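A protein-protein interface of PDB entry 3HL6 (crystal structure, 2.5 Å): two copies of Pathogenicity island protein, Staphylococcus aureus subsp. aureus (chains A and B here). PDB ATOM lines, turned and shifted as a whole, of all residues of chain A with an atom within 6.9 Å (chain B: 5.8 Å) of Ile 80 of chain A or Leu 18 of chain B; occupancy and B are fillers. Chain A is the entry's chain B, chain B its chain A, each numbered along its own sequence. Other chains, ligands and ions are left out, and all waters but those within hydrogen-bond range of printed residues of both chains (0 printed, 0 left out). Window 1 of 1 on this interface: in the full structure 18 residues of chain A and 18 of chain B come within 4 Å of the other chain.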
ATOM      1  N   ALA A  14       4.864  23.404  23.300  1.00  0.00           N
ATOM      2  CA  ALA A  14       4.124  22.453  24.142  1.00  0.00           C
ATOM      3  C   ALA A  14       3.204  21.638  23.262  1.00  0.00           C
ATOM      4  O   ALA A  14       3.199  20.426  23.360  1.00  0.00           O
ATOM      5  CB  ALA A  14       3.350  23.160  25.280  1.00  0.00           C
ATOM      6  N   LEU A  18       3.261  17.742  22.503  1.00  0.00           N
ATOM      7  CA  LEU A  18       2.128  16.886  22.856  1.00  0.00           C
ATOM      8  C   LEU A  18       1.812  15.973  21.683  1.00  0.00           C
ATOM      9  O   LEU A  18       1.544  14.792  21.852  1.00  0.00           O
ATOM     10  CB  LEU A  18       0.881  17.726  23.260  1.00  0.00           C
ATOM     11  CG  LEU A  18      -0.346  17.020  23.887  1.00  0.00           C
ATOM     12  CD1 LEU A  18       0.077  16.292  25.130  1.00  0.00           C
ATOM     13  CD2 LEU A  18      -1.528  17.983  24.232  1.00  0.00           C
ATOM     14  N   THR A  22       2.253  11.680  21.906  1.00  0.00           N
ATOM     15  CA  THR A  22       1.298  10.660  21.595  1.00  0.00           C
ATOM     16  C   THR A  22       1.733   9.918  20.342  1.00  0.00           C
ATOM     17  O   THR A  22       1.712   8.698  20.294  1.00  0.00           O
ATOM     18  CB  THR A  22      -0.070  11.276  21.383  1.00  0.00           C
ATOM     19  OG1 THR A  22      -0.006  12.118  20.222  1.00  0.00           O
ATOM     20  CG2 THR A  22      -0.461  12.093  22.603  1.00  0.00           C
ATOM     21  N   PRO A  73       1.985   8.960  30.265  1.00  0.00           N
ATOM     22  CA  PRO A  73       0.684   8.630  29.690  1.00  0.00           C
ATOM     23  C   PRO A  73      -0.516   9.215  30.446  1.00  0.00           C
ATOM     24  O   PRO A  73      -1.466   9.686  29.810  1.00  0.00           O
ATOM     25  CB  PRO A  73       0.624   7.108  29.737  1.00  0.00           C
ATOM     26  CG  PRO A  73       1.999   6.651  29.688  1.00  0.00           C
ATOM     27  CD  PRO A  73       3.017   7.778  29.976  1.00  0.00           C
ATOM     28  N   THR A  76      -0.396  14.238  31.105  1.00  0.00           N
ATOM     29  CA  THR A  76      -0.107  15.167  30.043  1.00  0.00           C
ATOM     30  C   THR A  76      -0.537  16.582  30.424  1.00  0.00           C
ATOM     31  O   THR A  76      -0.250  17.527  29.707  1.00  0.00           O
ATOM     32  CB  THR A  76      -0.816  14.772  28.752  1.00  0.00           C
ATOM     33  OG1 THR A  76      -2.109  14.235  29.067  1.00  0.00           O
ATOM     34  CG2 THR A  76       0.010  13.712  27.992  1.00  0.00           C
ATOM     35  N   GLU A  77      -1.227  16.729  31.553  1.00  0.00           N
ATOM     36  CA  GLU A  77      -1.743  18.024  31.943  1.00  0.00           C
ATOM     37  C   GLU A  77      -0.660  19.093  32.075  1.00  0.00           C
ATOM     38  O   GLU A  77      -0.934  20.258  31.853  1.00  0.00           O
ATOM     39  CB  GLU A  77      -2.541  17.911  33.230  1.00  0.00           C
ATOM     40  CG  GLU A  77      -1.685  17.670  34.438  1.00  0.00           C
ATOM     41  CD  GLU A  77      -1.413  16.197  34.629  1.00  0.00           C
ATOM     42  OE1 GLU A  77      -1.811  15.403  33.735  1.00  0.00           O
ATOM     43  OE2 GLU A  77      -0.822  15.824  35.665  1.00  0.00           O
ATOM     44  N   GLY A  78       0.561  18.728  32.441  1.00  0.00           N
ATOM     45  CA  GLY A  78       1.673  19.672  32.335  1.00  0.00           C
ATOM     46  C   GLY A  78       1.806  20.292  30.952  1.00  0.00           C
ATOM     47  O   GLY A  78       1.722  21.521  30.806  1.00  0.00           O
ATOM     48  N   LEU A  79       1.992  19.471  29.919  1.00  0.00           N
ATOM     49  CA  LEU A  79       2.096  20.007  28.556  1.00  0.00           C
ATOM     50  C   LEU A  79       0.858  20.859  28.156  1.00  0.00           C
ATOM     51  O   LEU A  79       0.990  21.971  27.608  1.00  0.00           O
ATOM     52  CB  LEU A  79       2.352  18.884  27.541  1.00  0.00           C
ATOM     53  CG  LEU A  79       3.767  18.310  27.602  1.00  0.00           C
ATOM     54  CD1 LEU A  79       4.017  17.253  26.530  1.00  0.00           C
ATOM     55  CD2 LEU A  79       4.795  19.405  27.507  1.00  0.00           C
ATOM     56  N   ILE A  80      -0.334  20.340  28.465  1.00  0.00           N
ATOM     57  CA  ILE A  80      -1.605  20.945  28.046  1.00  0.00           C
ATOM     58  C   ILE A  80      -1.778  22.298  28.722  1.00  0.00           C
ATOM     59  O   ILE A  80      -2.291  23.251  28.126  1.00  0.00           O
ATOM     60  CB  ILE A  80      -2.782  19.993  28.329  1.00  0.00           C
ATOM     61  CG1 ILE A  80      -2.436  18.608  27.793  1.00  0.00           C
ATOM     62  CG2 ILE A  80      -4.078  20.471  27.690  1.00  0.00           C
ATOM     63  CD1 ILE A  80      -3.571  17.723  27.676  1.00  0.00           C
ATOM     64  N   ARG A  81      -1.273  22.392  29.945  1.00  0.00           N
ATOM     65  CA  ARG A  81      -1.477  23.570  30.738  1.00  0.00           C
ATOM     66  C   ARG A  81      -0.575  24.689  30.308  1.00  0.00           C
ATOM     67  O   ARG A  81      -0.965  25.836  30.408  1.00  0.00           O
ATOM     68  CB  ARG A  81      -1.234  23.257  32.195  1.00  0.00           C
ATOM     69  CG  ARG A  81      -2.510  22.884  32.931  1.00  0.00           C
ATOM     70  CD  ARG A  81      -2.164  22.603  34.373  1.00  0.00           C
ATOM     71  NE  ARG A  81      -3.216  21.870  35.086  1.00  0.00           N
ATOM     72  CZ  ARG A  81      -2.984  21.035  36.106  1.00  0.00           C
ATOM     73  NH1 ARG A  81      -1.731  20.824  36.528  1.00  0.00           N
ATOM     74  NH2 ARG A  81      -4.001  20.408  36.708  1.00  0.00           N
ATOM     75  N   SER A  82       0.628  24.365  29.805  1.00  0.00           N
ATOM     76  CA  SER A  82       1.461  25.354  29.145  1.00  0.00           C
ATOM     77  C   SER A  82       0.844  25.843  27.853  1.00  0.00           C
ATOM     78  O   SER A  82       1.189  26.927  27.355  1.00  0.00           O
ATOM     79  CB  SER A  82       2.846  24.801  28.878  1.00  0.00           C
ATOM     80  OG  SER A  82       3.547  24.595  30.099  1.00  0.00           O
ATOM     81  N   ILE A  83      -0.062  25.062  27.281  1.00  0.00           N
ATOM     82  CA  ILE A  83      -0.669  25.518  26.032  1.00  0.00           C
ATOM     83  C   ILE A  83      -1.699  26.596  26.338  1.00  0.00           C
ATOM     84  O   ILE A  83      -1.630  27.717  25.823  1.00  0.00           O
ATOM     85  CB  ILE A  83      -1.321  24.374  25.224  1.00  0.00           C
ATOM     86  CG1 ILE A  83      -0.289  23.333  24.781  1.00  0.00           C
ATOM     87  CG2 ILE A  83      -2.010  24.929  23.998  1.00  0.00           C
ATOM     88  CD1 ILE A  83      -0.800  22.471  23.687  1.00  0.00           C
ATOM     89  N   GLU A  84      -2.632  26.269  27.220  1.00  0.00           N
ATOM     90  CA  GLU A  84      -3.544  27.261  27.775  1.00  0.00           C
ATOM     91  C   GLU A  84      -2.799  28.434  28.440  1.00  0.00           C
ATOM     92  O   GLU A  84      -3.103  29.606  28.216  1.00  0.00           O
ATOM     93  CB  GLU A  84      -4.529  26.564  28.732  1.00  0.00           C
ATOM     94  CG  GLU A  84      -5.245  25.360  28.050  1.00  0.00           C
ATOM     95  CD  GLU A  84      -6.636  25.066  28.635  1.00  0.00           C
ATOM     96  OE1 GLU A  84      -6.847  25.378  29.823  1.00  0.00           O
ATOM     97  OE2 GLU A  84      -7.518  24.538  27.903  1.00  0.00           O
ATOM     98  N   GLY A  85      -1.797  28.124  29.235  1.00  0.00           N
ATOM     99  CA  GLY A  85      -1.119  29.160  29.974  1.00  0.00           C
ATOM    100  C   GLY A  85      -0.440  30.151  29.054  1.00  0.00           C
ATOM    101  O   GLY A  85      -0.345  31.338  29.362  1.00  0.00           O
ATOM    102  N   HIS A  86       0.034  29.663  27.917  1.00  0.00           N
ATOM    103  CA  HIS A  86       0.747  30.508  26.965  1.00  0.00           C
ATOM    104  C   HIS A  86      -0.160  31.618  26.455  1.00  0.00           C
ATOM    105  O   HIS A  86       0.325  32.673  26.055  1.00  0.00           O
ATOM    106  CB  HIS A  86       1.275  29.666  25.789  1.00  0.00           C
ATOM    107  CG  HIS A  86       1.539  30.454  24.551  1.00  0.00           C
ATOM    108  ND1 HIS A  86       2.805  30.900  24.204  1.00  0.00           N
ATOM    109  CD2 HIS A  86       0.708  30.885  23.574  1.00  0.00           C
ATOM    110  CE1 HIS A  86       2.740  31.566  23.066  1.00  0.00           C
ATOM    111  NE2 HIS A  86       1.480  31.574  22.664  1.00  0.00           N
ATOM    112  N   PHE B  10      -9.662  21.709  32.320  1.00  0.00           N
ATOM    113  CA  PHE B  10      -8.902  22.754  31.633  1.00  0.00           C
ATOM    114  C   PHE B  10      -9.885  23.820  31.189  1.00  0.00           C
ATOM    115  O   PHE B  10     -11.096  23.606  31.219  1.00  0.00           O
ATOM    116  CB  PHE B  10      -8.138  22.156  30.422  1.00  0.00           C
ATOM    117  CG  PHE B  10      -7.129  21.068  30.799  1.00  0.00           C
ATOM    118  CD1 PHE B  10      -5.799  21.368  30.969  1.00  0.00           C
ATOM    119  CD2 PHE B  10      -7.529  19.758  30.993  1.00  0.00           C
ATOM    120  CE1 PHE B  10      -4.876  20.374  31.325  1.00  0.00           C
ATOM    121  CE2 PHE B  10      -6.626  18.771  31.356  1.00  0.00           C
ATOM    122  CZ  PHE B  10      -5.299  19.075  31.506  1.00  0.00           C
ATOM    123  N   ARG B  13     -12.570  22.039  26.560  1.00  0.00           N
ATOM    124  CA  ARG B  13     -12.847  20.633  26.463  1.00  0.00           C
ATOM    125  C   ARG B  13     -11.839  19.904  25.621  1.00  0.00           C
ATOM    126  O   ARG B  13     -11.492  18.773  25.941  1.00  0.00           O
ATOM    127  CB  ARG B  13     -14.271  20.387  25.941  1.00  0.00           C
ATOM    128  CG  ARG B  13     -15.334  20.779  26.989  1.00  0.00           C
ATOM    129  CD  ARG B  13     -16.755  20.545  26.515  1.00  0.00           C
ATOM    130  NE  ARG B  13     -17.018  21.061  25.169  1.00  0.00           N
ATOM    131  CZ  ARG B  13     -17.111  22.337  24.823  1.00  0.00           C
ATOM    132  NH1 ARG B  13     -16.940  23.288  25.708  1.00  0.00           N
ATOM    133  NH2 ARG B  13     -17.370  22.656  23.568  1.00  0.00           N
ATOM    134  N   ALA B  14     -11.360  20.543  24.547  1.00  0.00           N
ATOM    135  CA  ALA B  14     -10.295  19.951  23.695  1.00  0.00           C
ATOM    136  C   ALA B  14      -9.176  19.495  24.616  1.00  0.00           C
ATOM    137  O   ALA B  14      -8.683  18.381  24.514  1.00  0.00           O
ATOM    138  CB  ALA B  14      -9.792  20.968  22.716  1.00  0.00           C
ATOM    139  N   GLY B  15      -8.815  20.341  25.569  1.00  0.00           N
ATOM    140  CA  GLY B  15      -7.759  19.996  26.527  1.00  0.00           C
ATOM    141  C   GLY B  15      -8.019  18.778  27.389  1.00  0.00           C
ATOM    142  O   GLY B  15      -7.150  17.909  27.527  1.00  0.00           O
ATOM    143  N   THR B  16      -9.210  18.697  27.982  1.00  0.00           N
ATOM    144  CA  THR B  16      -9.532  17.571  28.851  1.00  0.00           C
ATOM    145  C   THR B  16      -9.577  16.321  28.010  1.00  0.00           C
ATOM    146  O   THR B  16      -8.985  15.288  28.378  1.00  0.00           O
ATOM    147  CB  THR B  16     -10.894  17.745  29.550  1.00  0.00           C
ATOM    148  OG1 THR B  16     -10.839  18.883  30.398  1.00  0.00           O
ATOM    149  CG2 THR B  16     -11.181  16.552  30.419  1.00  0.00           C
ATOM    150  N   LEU B  17     -10.266  16.422  26.866  1.00  0.00           N
ATOM    151  CA  LEU B  17     -10.308  15.303  25.908  1.00  0.00           C
ATOM    152  C   LEU B  17      -8.895  14.748  25.666  1.00  0.00           C
ATOM    153  O   LEU B  17      -8.704  13.537  25.724  1.00  0.00           O
ATOM    154  CB  LEU B  17     -10.990  15.678  24.603  1.00  0.00           C
ATOM    155  CG  LEU B  17     -12.516  15.477  24.591  1.00  0.00           C
ATOM    156  CD1 LEU B  17     -12.887  14.108  25.156  1.00  0.00           C
ATOM    157  CD2 LEU B  17     -13.154  16.481  25.459  1.00  0.00           C
ATOM    158  N   LEU B  18      -7.903  15.615  25.448  1.00  0.00           N
ATOM    159  CA  LEU B  18      -6.574  15.138  25.110  1.00  0.00           C
ATOM    160  C   LEU B  18      -5.909  14.486  26.295  1.00  0.00           C
ATOM    161  O   LEU B  18      -5.211  13.487  26.154  1.00  0.00           O
ATOM    162  CB  LEU B  18      -5.677  16.286  24.595  1.00  0.00           C
ATOM    163  CG  LEU B  18      -5.819  16.437  23.079  1.00  0.00           C
ATOM    164  CD1 LEU B  18      -5.840  17.905  22.640  1.00  0.00           C
ATOM    165  CD2 LEU B  18      -4.752  15.596  22.358  1.00  0.00           C
ATOM    166  N   ARG B  19      -6.108  15.041  27.485  1.00  0.00           N
ATOM    167  CA  ARG B  19      -5.519  14.392  28.658  1.00  0.00           C
ATOM    168  C   ARG B  19      -6.081  13.000  28.879  1.00  0.00           C
ATOM    169  O   ARG B  19      -5.405  12.123  29.421  1.00  0.00           O
ATOM    170  CB  ARG B  19      -5.691  15.214  29.930  1.00  0.00           C
ATOM    171  CG  ARG B  19      -5.150  14.489  31.171  1.00  0.00           C
ATOM    172  CD  ARG B  19      -5.407  15.283  32.439  1.00  0.00           C
ATOM    173  NE  ARG B  19      -4.694  14.661  33.558  1.00  0.00           N
ATOM    174  CZ  ARG B  19      -5.281  13.819  34.401  1.00  0.00           C
ATOM    175  NH1 ARG B  19      -6.586  13.539  34.234  1.00  0.00           N
ATOM    176  NH2 ARG B  19      -4.588  13.257  35.381  1.00  0.00           N
ATOM    177  N   TYR B  20      -7.327  12.790  28.488  1.00  0.00           N
ATOM    178  CA  TYR B  20      -7.932  11.493  28.782  1.00  0.00           C
ATOM    179  C   TYR B  20      -7.622  10.516  27.684  1.00  0.00           C
ATOM    180  O   TYR B  20      -7.388   9.325  27.920  1.00  0.00           O
ATOM    181  CB  TYR B  20      -9.435  11.607  29.081  1.00  0.00           C
ATOM    182  CG  TYR B  20      -9.579  11.993  30.516  1.00  0.00           C
ATOM    183  CD1 TYR B  20      -9.793  11.020  31.498  1.00  0.00           C
ATOM    184  CD2 TYR B  20      -9.395  13.308  30.912  1.00  0.00           C
ATOM    185  CE1 TYR B  20      -9.867  11.366  32.852  1.00  0.00           C
ATOM    186  CE2 TYR B  20      -9.475  13.677  32.256  1.00  0.00           C
ATOM    187  CZ  TYR B  20      -9.704  12.700  33.230  1.00  0.00           C
ATOM    188  OH  TYR B  20      -9.779  13.054  34.572  1.00  0.00           O
ATOM    189  N   TYR B  21      -7.568  11.059  26.479  1.00  0.00           N
ATOM    190  CA  TYR B  21      -7.288  10.257  25.331  1.00  0.00           C
ATOM    191  C   TYR B  21      -5.970   9.536  25.542  1.00  0.00           C
ATOM    192  O   TYR B  21      -5.893   8.326  25.417  1.00  0.00           O
ATOM    193  CB  TYR B  21      -7.259  11.121  24.077  1.00  0.00           C
ATOM    194  CG  TYR B  21      -6.730  10.381  22.890  1.00  0.00           C
ATOM    195  CD1 TYR B  21      -5.571  10.808  22.244  1.00  0.00           C
ATOM    196  CD2 TYR B  21      -7.364   9.231  22.437  1.00  0.00           C
ATOM    197  CE1 TYR B  21      -5.067  10.118  21.164  1.00  0.00           C
ATOM    198  CE2 TYR B  21      -6.862   8.522  21.372  1.00  0.00           C
ATOM    199  CZ  TYR B  21      -5.708   8.981  20.729  1.00  0.00           C
ATOM    200  OH  TYR B  21      -5.214   8.294  19.664  1.00  0.00           O
ATOM    201  N   THR B  22      -4.930  10.278  25.883  1.00  0.00           N
ATOM    202  CA  THR B  22      -3.610   9.682  25.936  1.00  0.00           C
ATOM    203  C   THR B  22      -3.456   8.932  27.245  1.00  0.00           C
ATOM    204  O   THR B  22      -2.639   8.032  27.363  1.00  0.00           O
ATOM    205  CB  THR B  22      -2.473  10.731  25.742  1.00  0.00           C
ATOM    206  OG1 THR B  22      -1.956  11.113  27.017  1.00  0.00           O
ATOM    207  CG2 THR B  22      -2.978  11.960  25.018  1.00  0.00           C
ATOM    208  N   GLY B  23      -4.269   9.293  28.230  1.00  0.00           N
ATOM    209  CA  GLY B  23      -4.361   8.521  29.465  1.00  0.00           C
ATOM    210  C   GLY B  23      -5.001   7.150  29.291  1.00  0.00           C
ATOM    211  O   GLY B  23      -4.591   6.191  29.940  1.00  0.00           O
ATOM    212  N   THR B  76      -3.358  13.810  16.727  1.00  0.00           N
ATOM    213  CA  THR B  76      -3.939  14.563  17.812  1.00  0.00           C
ATOM    214  C   THR B  76      -3.988  16.028  17.474  1.00  0.00           C
ATOM    215  O   THR B  76      -4.549  16.789  18.247  1.00  0.00           O
ATOM    216  CB  THR B  76      -3.136  14.377  19.107  1.00  0.00           C
ATOM    217  OG1 THR B  76      -1.740  14.507  18.801  1.00  0.00           O
ATOM    218  CG2 THR B  76      -3.402  12.970  19.708  1.00  0.00           C
ATOM    219  N   LEU B  79      -7.145  18.222  17.612  1.00  0.00           N
ATOM    220  CA  LEU B  79      -7.596  18.673  18.922  1.00  0.00           C
ATOM    221  C   LEU B  79      -6.726  19.818  19.484  1.00  0.00           C
ATOM    222  O   LEU B  79      -7.229  20.775  20.093  1.00  0.00           O
ATOM    223  CB  LEU B  79      -7.632  17.490  19.923  1.00  0.00           C
ATOM    224  CG  LEU B  79      -8.856  16.554  19.958  1.00  0.00           C
ATOM    225  CD1 LEU B  79      -8.786  15.530  21.126  1.00  0.00           C
ATOM    226  CD2 LEU B  79     -10.162  17.348  20.067  1.00  0.00           C
ATOM    227  N   ILE B  80      -5.414  19.689  19.332  1.00  0.00           N
ATOM    228  CA  ILE B  80      -4.505  20.729  19.776  1.00  0.00           C
ATOM    229  C   ILE B  80      -4.842  22.058  19.078  1.00  0.00           C
ATOM    230  O   ILE B  80      -4.634  23.148  19.623  1.00  0.00           O
ATOM    231  CB  ILE B  80      -3.072  20.297  19.466  1.00  0.00           C
ATOM    232  CG1 ILE B  80      -2.822  18.914  20.074  1.00  0.00           C
ATOM    233  CG2 ILE B  80      -2.068  21.305  19.981  1.00  0.00           C
ATOM    234  CD1 ILE B  80      -1.452  18.277  19.725  1.00  0.00           C
ATOM    235  N   ILE B  83      -7.469  23.915  20.689  1.00  0.00           N
ATOM    236  CA  ILE B  83      -7.001  24.683  21.834  1.00  0.00           C
ATOM    237  C   ILE B  83      -6.493  26.048  21.360  1.00  0.00           C
ATOM    238  O   ILE B  83      -6.964  27.077  21.811  1.00  0.00           O
ATOM    239  CB  ILE B  83      -5.944  23.941  22.661  1.00  0.00           C
ATOM    240  CG1 ILE B  83      -6.445  22.550  23.060  1.00  0.00           C
ATOM    241  CG2 ILE B  83      -5.607  24.747  23.881  1.00  0.00           C
ATOM    242  CD1 ILE B  83      -5.498  21.807  23.922  1.00  0.00           C
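The side-chain carboxylate (OE1) of Glu 77 of chain A is in salt-bridge range of the guanidinium group (NE) of Arg 19 of chain B (3.0 Å). The backbone carbonyl oxygen (O) of Pro 73 of chain A lies close to the backbone NH (N) of Gly 23 of chain B (3.2 Å). OG1 of Thr 22 of chain B sits at hydrogen-bond distance from O of Pro 73 of chain A (3.2 Å). OG1 of Thr 76 of chain B lies within hydrogen-bond range of OG1 of Thr 22 of chain A (3.3 Å).
O of Leu 18 of chain A sits close to OG1 of Thr 22 of chain A, 3.5 Å away. OH of Tyr 20 of chain B lies within hydrogen-bond range of NH1 of Arg 19 of chain B (3.2 Å).
Among the printed residues, pairs that only touch across the chains: Thr 76 of chain A with Thr 22 of chain B, Thr 76 of chain A with Arg 19 of chain B, Glu 77 of chain A with Phe 10 of chain B, Thr 22 of chain A with Thr 22 of chain B, Glu 84 of chain A with Phe 10 of chain B, Ile 80 of chain A with Gly 15 of chain B, Ile 83 of chain A with Ile 83 of chain B, Ile 80 of chain A with Phe 10 of chain B, Ile 80 of chain A with Arg 19 of chain B, Arg 81 of chain A with Phe 10 of chain B and Ile 80 of chain A with Leu 18 of chain B.
Of the printed residues of chain B, Ile 80 of chain A touches Phe 10 (3.7 Å), Gly 15 (3.6 Å), Leu 18 (3.999 Å) and Arg 19 (3.7 Å). Printed residues of chain A within 4 Å of Leu 18 of chain B: Ile 80 (3.999 Å). Of the printed residues of chain B, Thr 76 of chain A touches Arg 19 and Thr 22. Printed residues of chain A within 4 Å of Gly 15 of chain B: Ile 80. Of the printed residues of chain A, Arg 19 of chain B touches Thr 76, Glu 77 and Ile 80. Printed residues of chain A within 4 Å of Phe 10 of chain B: Glu 77 (3.5 Å), Ile 80 (3.7 Å), Arg 81 (3.8 Å) and Glu 84 (3.5 Å). Printed residues of chain A within 4 Å of Ile 83 of chain B: Ile 83 (3.6 Å). The nearest printed residue of chain B that does not touch Ile 80 of chain A is Ile 83 of chain B (4.2 Å). The nearest printed residue of chain A that does not touch Leu 18 of chain B is Thr 76 of chain A (4.3 Å).
Hydrophobic or aromatic side chains of chain A within 4 Å of the printed part of chain B: Ile 80 and Ile 83. Along chain A the printed residues that touch a printed residue of chain B span positions 22 to 84. Among the printed residues, 15 pairs touch across the chains. Among the printed residues, Asp or Glu carboxylates within 4 Å of a Lys or Arg side-chain nitrogen of the other chain: Glu 77 of chain A with Arg 19 of chain B.
Thr 22 of chain B touches its own counterpart, Thr 22 of chain A. Thr 22 of chain A touches Thr 76 of chain B, and with the chains exchanged Thr 76 of chain A touches Thr 22 of chain B. Ile 80 of chain A touches Leu 18 of chain B, but with the chains exchanged Leu 18 of chain A does not touch Ile 80 of chain B (4.3 Å). Ile 83 of chain A touches its own counterpart, Ile 83 of chain B. Of the 15 pairs that touch across the chains among the printed residues, 4 have their exchanged pair printed and touching as well.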
